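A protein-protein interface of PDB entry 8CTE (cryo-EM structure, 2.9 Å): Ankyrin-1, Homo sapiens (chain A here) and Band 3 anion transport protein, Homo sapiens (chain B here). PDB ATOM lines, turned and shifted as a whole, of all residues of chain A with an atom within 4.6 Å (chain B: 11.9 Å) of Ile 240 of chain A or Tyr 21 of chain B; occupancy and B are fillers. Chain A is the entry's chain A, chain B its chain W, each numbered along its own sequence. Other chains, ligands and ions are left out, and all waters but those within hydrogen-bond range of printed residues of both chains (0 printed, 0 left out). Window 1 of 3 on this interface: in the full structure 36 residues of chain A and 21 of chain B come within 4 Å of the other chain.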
ATOM      1  N   PHE A 207       9.606 -20.721 -10.206  1.00  0.00           N
ATOM      2  CA  PHE A 207       9.174 -20.122 -11.459  1.00  0.00           C
ATOM      3  C   PHE A 207       9.261 -21.123 -12.604  1.00  0.00           C
ATOM      4  O   PHE A 207      10.232 -21.872 -12.731  1.00  0.00           O
ATOM      5  CB  PHE A 207      10.011 -18.886 -11.788  1.00  0.00           C
ATOM      6  CG  PHE A 207       9.623 -17.666 -11.004  1.00  0.00           C
ATOM      7  CD1 PHE A 207       8.294 -17.410 -10.711  1.00  0.00           C
ATOM      8  CD2 PHE A 207      10.585 -16.780 -10.553  1.00  0.00           C
ATOM      9  CE1 PHE A 207       7.933 -16.287  -9.989  1.00  0.00           C
ATOM     10  CE2 PHE A 207      10.230 -15.657  -9.831  1.00  0.00           C
ATOM     11  CZ  PHE A 207       8.903 -15.411  -9.548  1.00  0.00           C
ATOM     12  N   HIS A 211       7.924 -18.101 -17.157  1.00  0.00           N
ATOM     13  CA  HIS A 211       8.338 -16.881 -16.471  1.00  0.00           C
ATOM     14  C   HIS A 211       9.649 -16.350 -17.036  1.00  0.00           C
ATOM     15  O   HIS A 211       9.793 -15.142 -17.255  1.00  0.00           O
ATOM     16  CB  HIS A 211       8.470 -17.133 -14.969  1.00  0.00           C
ATOM     17  CG  HIS A 211       7.160 -17.316 -14.266  1.00  0.00           C
ATOM     18  ND1 HIS A 211       6.439 -18.487 -14.329  1.00  0.00           N
ATOM     19  CD2 HIS A 211       6.447 -16.477 -13.478  1.00  0.00           C
ATOM     20  CE1 HIS A 211       5.336 -18.362 -13.615  1.00  0.00           C
ATOM     21  NE2 HIS A 211       5.317 -17.151 -13.088  1.00  0.00           N
ATOM     22  N   PHE A 234       0.110 -19.316 -14.329  1.00  0.00           N
ATOM     23  CA  PHE A 234       0.735 -20.081 -13.259  1.00  0.00           C
ATOM     24  C   PHE A 234       1.145 -19.114 -12.158  1.00  0.00           C
ATOM     25  O   PHE A 234       1.932 -18.191 -12.397  1.00  0.00           O
ATOM     26  CB  PHE A 234       1.941 -20.868 -13.771  1.00  0.00           C
ATOM     27  CG  PHE A 234       2.465 -21.875 -12.785  1.00  0.00           C
ATOM     28  CD1 PHE A 234       3.435 -21.522 -11.861  1.00  0.00           C
ATOM     29  CD2 PHE A 234       1.983 -23.173 -12.782  1.00  0.00           C
ATOM     30  CE1 PHE A 234       3.915 -22.449 -10.953  1.00  0.00           C
ATOM     31  CE2 PHE A 234       2.460 -24.102 -11.878  1.00  0.00           C
ATOM     32  CZ  PHE A 234       3.426 -23.739 -10.962  1.00  0.00           C
ATOM     33  N   PRO A 236       2.908 -18.667  -8.584  1.00  0.00           N
ATOM     34  CA  PRO A 236       3.709 -19.218  -7.483  1.00  0.00           C
ATOM     35  C   PRO A 236       3.270 -18.674  -6.133  1.00  0.00           C
ATOM     36  O   PRO A 236       2.257 -17.973  -6.038  1.00  0.00           O
ATOM     37  CB  PRO A 236       5.140 -18.776  -7.829  1.00  0.00           C
ATOM     38  CG  PRO A 236       5.094 -18.387  -9.279  1.00  0.00           C
ATOM     39  CD  PRO A 236       3.718 -17.851  -9.500  1.00  0.00           C
ATOM     40  N   ASN A 238       4.625 -16.386  -4.363  1.00  0.00           N
ATOM     41  CA  ASN A 238       4.732 -14.934  -4.345  1.00  0.00           C
ATOM     42  C   ASN A 238       3.655 -14.244  -5.173  1.00  0.00           C
ATOM     43  O   ASN A 238       3.510 -13.021  -5.076  1.00  0.00           O
ATOM     44  CB  ASN A 238       6.118 -14.497  -4.836  1.00  0.00           C
ATOM     45  CG  ASN A 238       6.514 -15.158  -6.145  1.00  0.00           C
ATOM     46  OD1 ASN A 238       5.677 -15.693  -6.870  1.00  0.00           O
ATOM     47  ND2 ASN A 238       7.804 -15.119  -6.454  1.00  0.00           N
ATOM     48  N   GLY A 239       2.904 -14.993  -5.978  1.00  0.00           N
ATOM     49  CA  GLY A 239       1.838 -14.419  -6.772  1.00  0.00           C
ATOM     50  C   GLY A 239       2.271 -13.746  -8.052  1.00  0.00           C
ATOM     51  O   GLY A 239       1.467 -13.025  -8.652  1.00  0.00           O
ATOM     52  N   ILE A 240       3.504 -13.961  -8.498  1.00  0.00           N
ATOM     53  CA  ILE A 240       4.040 -13.274  -9.668  1.00  0.00           C
ATOM     54  C   ILE A 240       3.742 -14.118 -10.902  1.00  0.00           C
ATOM     55  O   ILE A 240       4.405 -15.127 -11.154  1.00  0.00           O
ATOM     56  CB  ILE A 240       5.542 -13.011  -9.524  1.00  0.00           C
ATOM     57  CG1 ILE A 240       5.824 -12.260  -8.221  1.00  0.00           C
ATOM     58  CG2 ILE A 240       6.056 -12.220 -10.712  1.00  0.00           C
ATOM     59  CD1 ILE A 240       7.293 -12.021  -7.958  1.00  0.00           C
ATOM     60  N   THR A 241       2.749 -13.698 -11.677  1.00  0.00           N
ATOM     61  CA  THR A 241       2.395 -14.365 -12.918  1.00  0.00           C
ATOM     62  C   THR A 241       3.351 -13.953 -14.034  1.00  0.00           C
ATOM     63  O   THR A 241       4.058 -12.949 -13.917  1.00  0.00           O
ATOM     64  CB  THR A 241       0.958 -14.024 -13.302  1.00  0.00           C
ATOM     65  OG1 THR A 241       0.826 -12.608 -13.468  1.00  0.00           O
ATOM     66  CG2 THR A 241      -0.002 -14.498 -12.223  1.00  0.00           C
ATOM     67  N   PRO A 242       3.419 -14.735 -15.121  1.00  0.00           N
ATOM     68  CA  PRO A 242       4.206 -14.282 -16.283  1.00  0.00           C
ATOM     69  C   PRO A 242       3.733 -12.952 -16.845  1.00  0.00           C
ATOM     70  O   PRO A 242       4.544 -12.188 -17.384  1.00  0.00           O
ATOM     71  CB  PRO A 242       4.026 -15.427 -17.289  1.00  0.00           C
ATOM     72  CG  PRO A 242       3.776 -16.624 -16.443  1.00  0.00           C
ATOM     73  CD  PRO A 242       2.971 -16.131 -15.275  1.00  0.00           C
ATOM     74  N   HIS A 244       2.696 -10.478 -15.004  1.00  0.00           N
ATOM     75  CA  HIS A 244       3.338  -9.493 -14.138  1.00  0.00           C
ATOM     76  C   HIS A 244       4.770  -9.219 -14.578  1.00  0.00           C
ATOM     77  O   HIS A 244       5.193  -8.058 -14.651  1.00  0.00           O
ATOM     78  CB  HIS A 244       3.323  -9.970 -12.685  1.00  0.00           C
ATOM     79  CG  HIS A 244       2.007  -9.793 -11.995  1.00  0.00           C
ATOM     80  ND1 HIS A 244       0.999 -10.730 -12.064  1.00  0.00           N
ATOM     81  CD2 HIS A 244       1.539  -8.793 -11.213  1.00  0.00           C
ATOM     82  CE1 HIS A 244      -0.036 -10.312 -11.358  1.00  0.00           C
ATOM     83  NE2 HIS A 244       0.266  -9.138 -10.832  1.00  0.00           N
ATOM     84  N   ILE A 245       5.528 -10.275 -14.883  1.00  0.00           N
ATOM     85  CA  ILE A 245       6.916 -10.108 -15.304  1.00  0.00           C
ATOM     86  C   ILE A 245       6.982  -9.373 -16.637  1.00  0.00           C
ATOM     87  O   ILE A 245       7.818  -8.484 -16.836  1.00  0.00           O
ATOM     88  CB  ILE A 245       7.625 -11.472 -15.379  1.00  0.00           C
ATOM     89  CG1 ILE A 245       7.511 -12.207 -14.043  1.00  0.00           C
ATOM     90  CG2 ILE A 245       9.082 -11.293 -15.752  1.00  0.00           C
ATOM     91  CD1 ILE A 245       8.277 -13.511 -13.993  1.00  0.00           C
ATOM     92  N   ARG A 248       6.202  -5.711 -16.042  1.00  0.00           N
ATOM     93  CA  ARG A 248       7.271  -5.014 -15.333  1.00  0.00           C
ATOM     94  C   ARG A 248       8.484  -4.793 -16.232  1.00  0.00           C
ATOM     95  O   ARG A 248       9.125  -3.738 -16.168  1.00  0.00           O
ATOM     96  CB  ARG A 248       7.660  -5.800 -14.079  1.00  0.00           C
ATOM     97  CG  ARG A 248       8.211  -4.957 -12.932  1.00  0.00           C
ATOM     98  CD  ARG A 248       9.707  -4.712 -13.061  1.00  0.00           C
ATOM     99  NE  ARG A 248      10.460  -5.959 -13.121  1.00  0.00           N
ATOM    100  CZ  ARG A 248      11.779  -6.035 -13.232  1.00  0.00           C
ATOM    101  NH1 ARG A 248      12.530  -4.948 -13.300  1.00  0.00           N
ATOM    102  NH2 ARG A 248      12.358  -7.231 -13.276  1.00  0.00           N
ATOM    103  N   THR A 269      -0.402 -10.053  -6.659  1.00  0.00           N
ATOM    104  CA  THR A 269       0.736 -10.723  -6.042  1.00  0.00           C
ATOM    105  C   THR A 269       0.512 -10.806  -4.531  1.00  0.00           C
ATOM    106  O   THR A 269      -0.573 -10.519  -4.019  1.00  0.00           O
ATOM    107  CB  THR A 269       2.030  -9.992  -6.386  1.00  0.00           C
ATOM    108  OG1 THR A 269       1.993  -8.666  -5.842  1.00  0.00           O
ATOM    109  CG2 THR A 269       2.206  -9.904  -7.891  1.00  0.00           C
ATOM    110  N   ASP A 271       1.843  -8.836  -2.436  1.00  0.00           N
ATOM    111  CA  ASP A 271       1.655  -7.445  -2.044  1.00  0.00           C
ATOM    112  C   ASP A 271       0.477  -6.806  -2.767  1.00  0.00           C
ATOM    113  O   ASP A 271       0.339  -5.578  -2.745  1.00  0.00           O
ATOM    114  CB  ASP A 271       2.932  -6.642  -2.298  1.00  0.00           C
ATOM    115  CG  ASP A 271       4.032  -6.965  -1.307  1.00  0.00           C
ATOM    116  OD1 ASP A 271       4.552  -8.100  -1.335  1.00  0.00           O
ATOM    117  OD2 ASP A 271       4.377  -6.080  -0.496  1.00  0.00           O
ATOM    118  N   LEU A 273      -0.136  -6.464  -6.005  1.00  0.00           N
ATOM    119  CA  LEU A 273       0.252  -5.645  -7.145  1.00  0.00           C
ATOM    120  C   LEU A 273      -0.315  -6.252  -8.422  1.00  0.00           C
ATOM    121  O   LEU A 273       0.045  -7.373  -8.798  1.00  0.00           O
ATOM    122  CB  LEU A 273       1.773  -5.527  -7.245  1.00  0.00           C
ATOM    123  CG  LEU A 273       2.414  -4.256  -6.688  1.00  0.00           C
ATOM    124  CD1 LEU A 273       2.556  -4.332  -5.178  1.00  0.00           C
ATOM    125  CD2 LEU A 273       3.757  -3.999  -7.347  1.00  0.00           C
ATOM    126  N   CYS A 278       2.660  -2.864 -11.974  1.00  0.00           N
ATOM    127  CA  CYS A 278       4.017  -3.127 -12.444  1.00  0.00           C
ATOM    128  C   CYS A 278       4.345  -2.299 -13.679  1.00  0.00           C
ATOM    129  O   CYS A 278       5.465  -1.795 -13.819  1.00  0.00           O
ATOM    130  CB  CYS A 278       4.191  -4.618 -12.736  1.00  0.00           C
ATOM    131  SG  CYS A 278       3.831  -5.702 -11.336  1.00  0.00           S
ATOM    132  N   ARG A 281       4.648   1.563 -12.439  1.00  0.00           N
ATOM    133  CA  ARG A 281       5.812   1.922 -11.638  1.00  0.00           C
ATOM    134  C   ARG A 281       7.094   1.950 -12.459  1.00  0.00           C
ATOM    135  O   ARG A 281       8.080   2.553 -12.020  1.00  0.00           O
ATOM    136  CB  ARG A 281       5.964   0.960 -10.458  1.00  0.00           C
ATOM    137  CG  ARG A 281       6.379  -0.449 -10.834  1.00  0.00           C
ATOM    138  CD  ARG A 281       6.403  -1.341  -9.604  1.00  0.00           C
ATOM    139  NE  ARG A 281       7.137  -0.727  -8.504  1.00  0.00           N
ATOM    140  CZ  ARG A 281       7.277  -1.267  -7.301  1.00  0.00           C
ATOM    141  NH1 ARG A 281       6.743  -2.440  -7.005  1.00  0.00           N
ATOM    142  NH2 ARG A 281       7.967  -0.612  -6.372  1.00  0.00           N
ATOM    143  N   MET B  12      19.907 -16.446 -11.512  1.00  0.00           N
ATOM    144  CA  MET B  12      18.604 -16.253 -12.141  1.00  0.00           C
ATOM    145  C   MET B  12      17.624 -15.583 -11.185  1.00  0.00           C
ATOM    146  O   MET B  12      16.836 -14.723 -11.598  1.00  0.00           O
ATOM    147  CB  MET B  12      18.050 -17.591 -12.630  1.00  0.00           C
ATOM    148  CG  MET B  12      16.696 -17.483 -13.314  1.00  0.00           C
ATOM    149  SD  MET B  12      16.700 -16.298 -14.673  1.00  0.00           S
ATOM    150  CE  MET B  12      17.896 -17.045 -15.776  1.00  0.00           C
ATOM    151  N   GLU B  13      17.656 -15.964  -9.905  1.00  0.00           N
ATOM    152  CA  GLU B  13      16.799 -15.320  -8.914  1.00  0.00           C
ATOM    153  C   GLU B  13      17.145 -13.845  -8.765  1.00  0.00           C
ATOM    154  O   GLU B  13      16.252 -13.000  -8.627  1.00  0.00           O
ATOM    155  CB  GLU B  13      16.924 -16.041  -7.571  1.00  0.00           C
ATOM    156  CG  GLU B  13      16.033 -15.483  -6.474  1.00  0.00           C
ATOM    157  CD  GLU B  13      16.183 -16.233  -5.165  1.00  0.00           C
ATOM    158  OE1 GLU B  13      16.992 -17.185  -5.115  1.00  0.00           O
ATOM    159  OE2 GLU B  13      15.494 -15.875  -4.187  1.00  0.00           O
ATOM    160  N   GLU B  14      18.440 -13.517  -8.783  1.00  0.00           N
ATOM    161  CA  GLU B  14      18.852 -12.118  -8.731  1.00  0.00           C
ATOM    162  C   GLU B  14      18.401 -11.358  -9.974  1.00  0.00           C
ATOM    163  O   GLU B  14      17.976 -10.200  -9.884  1.00  0.00           O
ATOM    164  CB  GLU B  14      20.369 -12.023  -8.568  1.00  0.00           C
ATOM    165  CG  GLU B  14      20.882 -12.448  -7.201  1.00  0.00           C
ATOM    166  CD  GLU B  14      20.604 -11.416  -6.124  1.00  0.00           C
ATOM    167  OE1 GLU B  14      20.325 -10.248  -6.469  1.00  0.00           O
ATOM    168  OE2 GLU B  14      20.666 -11.774  -4.928  1.00  0.00           O
ATOM    169  N   ASN B  15      18.491 -11.993 -11.146  1.00  0.00           N
ATOM    170  CA  ASN B  15      18.114 -11.325 -12.389  1.00  0.00           C
ATOM    171  C   ASN B  15      16.611 -11.084 -12.465  1.00  0.00           C
ATOM    172  O   ASN B  15      16.169 -10.048 -12.977  1.00  0.00           O
ATOM    173  CB  ASN B  15      18.583 -12.146 -13.590  1.00  0.00           C
ATOM    174  CG  ASN B  15      20.092 -12.182 -13.719  1.00  0.00           C
ATOM    175  OD1 ASN B  15      20.782 -11.233 -13.347  1.00  0.00           O
ATOM    176  ND2 ASN B  15      20.613 -13.282 -14.249  1.00  0.00           N
ATOM    177  N   LEU B  16      15.809 -12.031 -11.969  1.00  0.00           N
ATOM    178  CA  LEU B  16      14.358 -11.896 -12.061  1.00  0.00           C
ATOM    179  C   LEU B  16      13.836 -10.751 -11.201  1.00  0.00           C
ATOM    180  O   LEU B  16      12.775 -10.191 -11.504  1.00  0.00           O
ATOM    181  CB  LEU B  16      13.686 -13.212 -11.674  1.00  0.00           C
ATOM    182  CG  LEU B  16      13.818 -14.322 -12.720  1.00  0.00           C
ATOM    183  CD1 LEU B  16      13.551 -15.683 -12.105  1.00  0.00           C
ATOM    184  CD2 LEU B  16      12.882 -14.067 -13.891  1.00  0.00           C
ATOM    185  N   GLU B  17      14.561 -10.394 -10.138  1.00  0.00           N
ATOM    186  CA  GLU B  17      14.257  -9.237  -9.294  1.00  0.00           C
ATOM    187  C   GLU B  17      12.848  -9.328  -8.702  1.00  0.00           C
ATOM    188  O   GLU B  17      11.961  -8.526  -8.999  1.00  0.00           O
ATOM    189  CB  GLU B  17      14.452  -7.928 -10.069  1.00  0.00           C
ATOM    190  CG  GLU B  17      15.883  -7.689 -10.526  1.00  0.00           C
ATOM    191  CD  GLU B  17      16.051  -6.371 -11.255  1.00  0.00           C
ATOM    192  OE1 GLU B  17      15.035  -5.682 -11.484  1.00  0.00           O
ATOM    193  OE2 GLU B  17      17.201  -6.022 -11.598  1.00  0.00           O
ATOM    194  N   GLN B  18      12.658 -10.339  -7.851  1.00  0.00           N
ATOM    195  CA  GLN B  18      11.368 -10.552  -7.207  1.00  0.00           C
ATOM    196  C   GLN B  18      11.006  -9.427  -6.245  1.00  0.00           C
ATOM    197  O   GLN B  18       9.827  -9.273  -5.906  1.00  0.00           O
ATOM    198  CB  GLN B  18      11.374 -11.894  -6.475  1.00  0.00           C
ATOM    199  CG  GLN B  18      11.756 -13.068  -7.363  1.00  0.00           C
ATOM    200  CD  GLN B  18      12.143 -14.301  -6.572  1.00  0.00           C
ATOM    201  OE1 GLN B  18      12.651 -15.275  -7.128  1.00  0.00           O
ATOM    202  NE2 GLN B  18      11.906 -14.267  -5.266  1.00  0.00           N
ATOM    203  N   GLU B  19      11.988  -8.641  -5.798  1.00  0.00           N
ATOM    204  CA  GLU B  19      11.694  -7.519  -4.912  1.00  0.00           C
ATOM    205  C   GLU B  19      10.995  -6.383  -5.649  1.00  0.00           C
ATOM    206  O   GLU B  19      10.329  -5.556  -5.017  1.00  0.00           O
ATOM    207  CB  GLU B  19      12.981  -7.014  -4.260  1.00  0.00           C
ATOM    208  N   GLU B  20      11.136  -6.322  -6.975  1.00  0.00           N
ATOM    209  CA  GLU B  20      10.497  -5.273  -7.760  1.00  0.00           C
ATOM    210  C   GLU B  20       8.989  -5.460  -7.887  1.00  0.00           C
ATOM    211  O   GLU B  20       8.306  -4.536  -8.339  1.00  0.00           O
ATOM    212  CB  GLU B  20      11.123  -5.207  -9.155  1.00  0.00           C
ATOM    213  CG  GLU B  20      12.603  -4.851  -9.162  1.00  0.00           C
ATOM    214  CD  GLU B  20      12.864  -3.404  -8.788  1.00  0.00           C
ATOM    215  OE1 GLU B  20      11.941  -2.573  -8.928  1.00  0.00           O
ATOM    216  OE2 GLU B  20      13.993  -3.096  -8.355  1.00  0.00           O
ATOM    217  N   TYR B  21       8.460  -6.620  -7.503  1.00  0.00           N
ATOM    218  CA  TYR B  21       7.035  -6.902  -7.589  1.00  0.00           C
ATOM    219  C   TYR B  21       6.323  -6.723  -6.256  1.00  0.00           C
ATOM    220  O   TYR B  21       5.150  -7.090  -6.134  1.00  0.00           O
ATOM    221  CB  TYR B  21       6.812  -8.322  -8.115  1.00  0.00           C
ATOM    222  CG  TYR B  21       7.463  -8.585  -9.452  1.00  0.00           C
ATOM    223  CD1 TYR B  21       6.782  -8.346 -10.638  1.00  0.00           C
ATOM    224  CD2 TYR B  21       8.762  -9.072  -9.529  1.00  0.00           C
ATOM    225  CE1 TYR B  21       7.375  -8.585 -11.862  1.00  0.00           C
ATOM    226  CE2 TYR B  21       9.364  -9.313 -10.747  1.00  0.00           C
ATOM    227  CZ  TYR B  21       8.666  -9.067 -11.910  1.00  0.00           C
ATOM    228  OH  TYR B  21       9.265  -9.308 -13.124  1.00  0.00           O
ATOM    229  N   GLU B  22       7.001  -6.168  -5.257  1.00  0.00           N
ATOM    230  CA  GLU B  22       6.437  -5.960  -3.935  1.00  0.00           C
ATOM    231  C   GLU B  22       6.350  -4.470  -3.634  1.00  0.00           C
ATOM    232  O   GLU B  22       7.145  -3.670  -4.138  1.00  0.00           O
ATOM    233  CB  GLU B  22       7.284  -6.647  -2.860  1.00  0.00           C
ATOM    234  CG  GLU B  22       7.838  -7.999  -3.268  1.00  0.00           C
ATOM    235  CD  GLU B  22       8.775  -8.579  -2.228  1.00  0.00           C
ATOM    236  OE1 GLU B  22       8.626  -8.235  -1.036  1.00  0.00           O
ATOM    237  OE2 GLU B  22       9.664  -9.373  -2.600  1.00  0.00           O
ATOM    238  N   ASP B  23       5.373  -4.102  -2.806  1.00  0.00           N
ATOM    239  CA  ASP B  23       5.260  -2.731  -2.331  1.00  0.00           C
ATOM    240  C   ASP B  23       6.236  -2.559  -1.176  1.00  0.00           C
ATOM    241  O   ASP B  23       6.065  -3.210  -0.133  1.00  0.00           O
ATOM    242  CB  ASP B  23       3.835  -2.432  -1.883  1.00  0.00           C
ATOM    243  CG  ASP B  23       3.522  -0.948  -1.876  1.00  0.00           C
ATOM    244  OD1 ASP B  23       4.445  -0.136  -1.652  1.00  0.00           O
ATOM    245  OD2 ASP B  23       2.346  -0.590  -2.095  1.00  0.00           O
ATOM    246  N   PRO B  24       7.270  -1.722  -1.311  1.00  0.00           N
ATOM    247  CA  PRO B  24       8.302  -1.671  -0.257  1.00  0.00           C
ATOM    248  C   PRO B  24       7.798  -1.125   1.067  1.00  0.00           C
ATOM    249  O   PRO B  24       7.897  -1.810   2.094  1.00  0.00           O
ATOM    250  CB  PRO B  24       9.383  -0.769  -0.876  1.00  0.00           C
ATOM    251  CG  PRO B  24       9.098  -0.761  -2.350  1.00  0.00           C
ATOM    252  CD  PRO B  24       7.614  -0.879  -2.466  1.00  0.00           C
ATOM    253  N   ASP B  25       7.240   0.084   1.066  1.00  0.00           N
ATOM    254  CA  ASP B  25       6.784   0.741   2.285  1.00  0.00           C
ATOM    255  C   ASP B  25       6.015   1.995   1.899  1.00  0.00           C
ATOM    256  O   ASP B  25       5.910   2.341   0.718  1.00  0.00           O
ATOM    257  CB  ASP B  25       7.952   1.100   3.213  1.00  0.00           C
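The backbone carbonyl oxygen (O) of Leu 16 of chain B lies within hydrogen-bond range of the guanidinium group (NH2) of Arg 248 of chain A (3.5 Å).
OE1 of Glu 17 of chain B lies within salt-bridge range of NH1 of Arg 248 of chain A, at 3.2 Å.
The side-chain carboxylate of Asp 271 of chain A is in hydrogen-bond range of the backbone NH of Asp 23 of chain B (3.2 Å).
The guanidinium group (NH1) of Arg 281 of chain A lies within hydrogen-bond range of the backbone carbonyl oxygen (O) of Glu 20 of chain B.
NH1 of Arg 281 of chain A sits at hydrogen-bond distance from O of Glu 22 of chain B (3.1 Å).
A ring nitrogen (NE2) of His 211 of chain A is in hydrogen-bond range of the backbone carbonyl oxygen of Ile 240 of chain A (2.9 Å).
The backbone NH of Ile 240 of chain A sits at hydrogen-bond distance from the side-chain amide oxygen of Asn 238 of chain A, 3.2 Å away.
OG1 of Thr 241 of chain A sits at hydrogen-bond distance from N of His 244 of chain A.
The backbone carbonyl oxygen of Leu 273 of chain A sits at hydrogen-bond distance from a ring nitrogen (NE2) of His 244 of chain A (2.7 Å).
The side-chain hydroxyl of Thr 269 of chain A sits close to the backbone NH of Asp 271 of chain A (3.4 Å).
The side-chain hydroxyl (OG1) of Thr 269 of chain A sits at hydrogen-bond distance from the backbone NH (N) of Leu 273 of chain A, 3.1 Å away.
CD1 of Leu 16 of chain B touches CD2 of Phe 207 of chain A, at 3.5 Å.
Gln 18 of chain B touches Phe 207 of chain A (OE1 to CE2, 3.6 Å).
Ile 240 of chain A touches Tyr 21 of chain B.
O of His 244 of chain A touches CE1 of Tyr 21 of chain B (3.6 Å).
CG2 of Ile 245 of chain A touches OH of Tyr 21 of chain B (3.3 Å).
NE of Arg 248 of chain A touches OH of Tyr 21 of chain B, 3.6 Å away.
OD1 of Asp 271 of chain A touches CB of Glu 22 of chain B, at 3.4 Å.
Leu 273 of chain A touches Tyr 21 of chain B.
Leu 273 of chain A touches Asp 23 of chain B.
Pro 24 of chain B touches Arg 281 of chain A.
Ile 240 of chain A touches just one residue of chain B: Tyr 21.
No residue of chain B comes within 4 Å of Pro 236 of chain A.
No residue of chain B comes within 4 Å of Asn 238 of chain A.
No residue of chain B comes within 4 Å of Pro 242 of chain A.
His 244 of chain A touches just one residue of chain B: Tyr 21.
Of the printed residues of chain B, Ile 245 of chain A touches Tyr 21 (3.3 Å).
Arg 248 of chain A touches just these residues of chain B: Leu 16, Glu 17 and Tyr 21.
Of chain B, only Glu 22 (3.4 Å) and Asp 23 (3.2 Å) come within 4 Å of Asp 271 of chain A.
Of chain B, only Tyr 21 and Asp 23 come within 4 Å of Leu 273 of chain A.
No residue of chain B comes within 4 Å of Cys 278 of chain A.
Of the printed residues of chain A, Glu 17 of chain B touches Arg 248 (3.2 Å).
Of the printed residues of chain A, Glu 20 of chain B touches Arg 281 (2.9 Å).
Of the printed residues of chain A, Glu 22 of chain B touches Asp 271 (3.4 Å) and Arg 281 (3.1 Å).
The nearest residue of chain B that does not touch Ile 240 of chain A is Gln 18 of chain B (4.3 Å).
The nearest residue of chain A that does not touch Tyr 21 of chain B is Cys 278 of chain A (4.02 Å).
Of the 14 printed residues of chain B, 8 touch a printed residue of chain A.
Hydrophobic or aromatic side chains of chain B that line the printed part of chain A: Leu 16, Tyr 21 and Pro 24.
Hydrophobic or aromatic side chains of chain A that line the printed part of chain B: Phe 207, Ile 240, Ile 245 and Leu 273.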
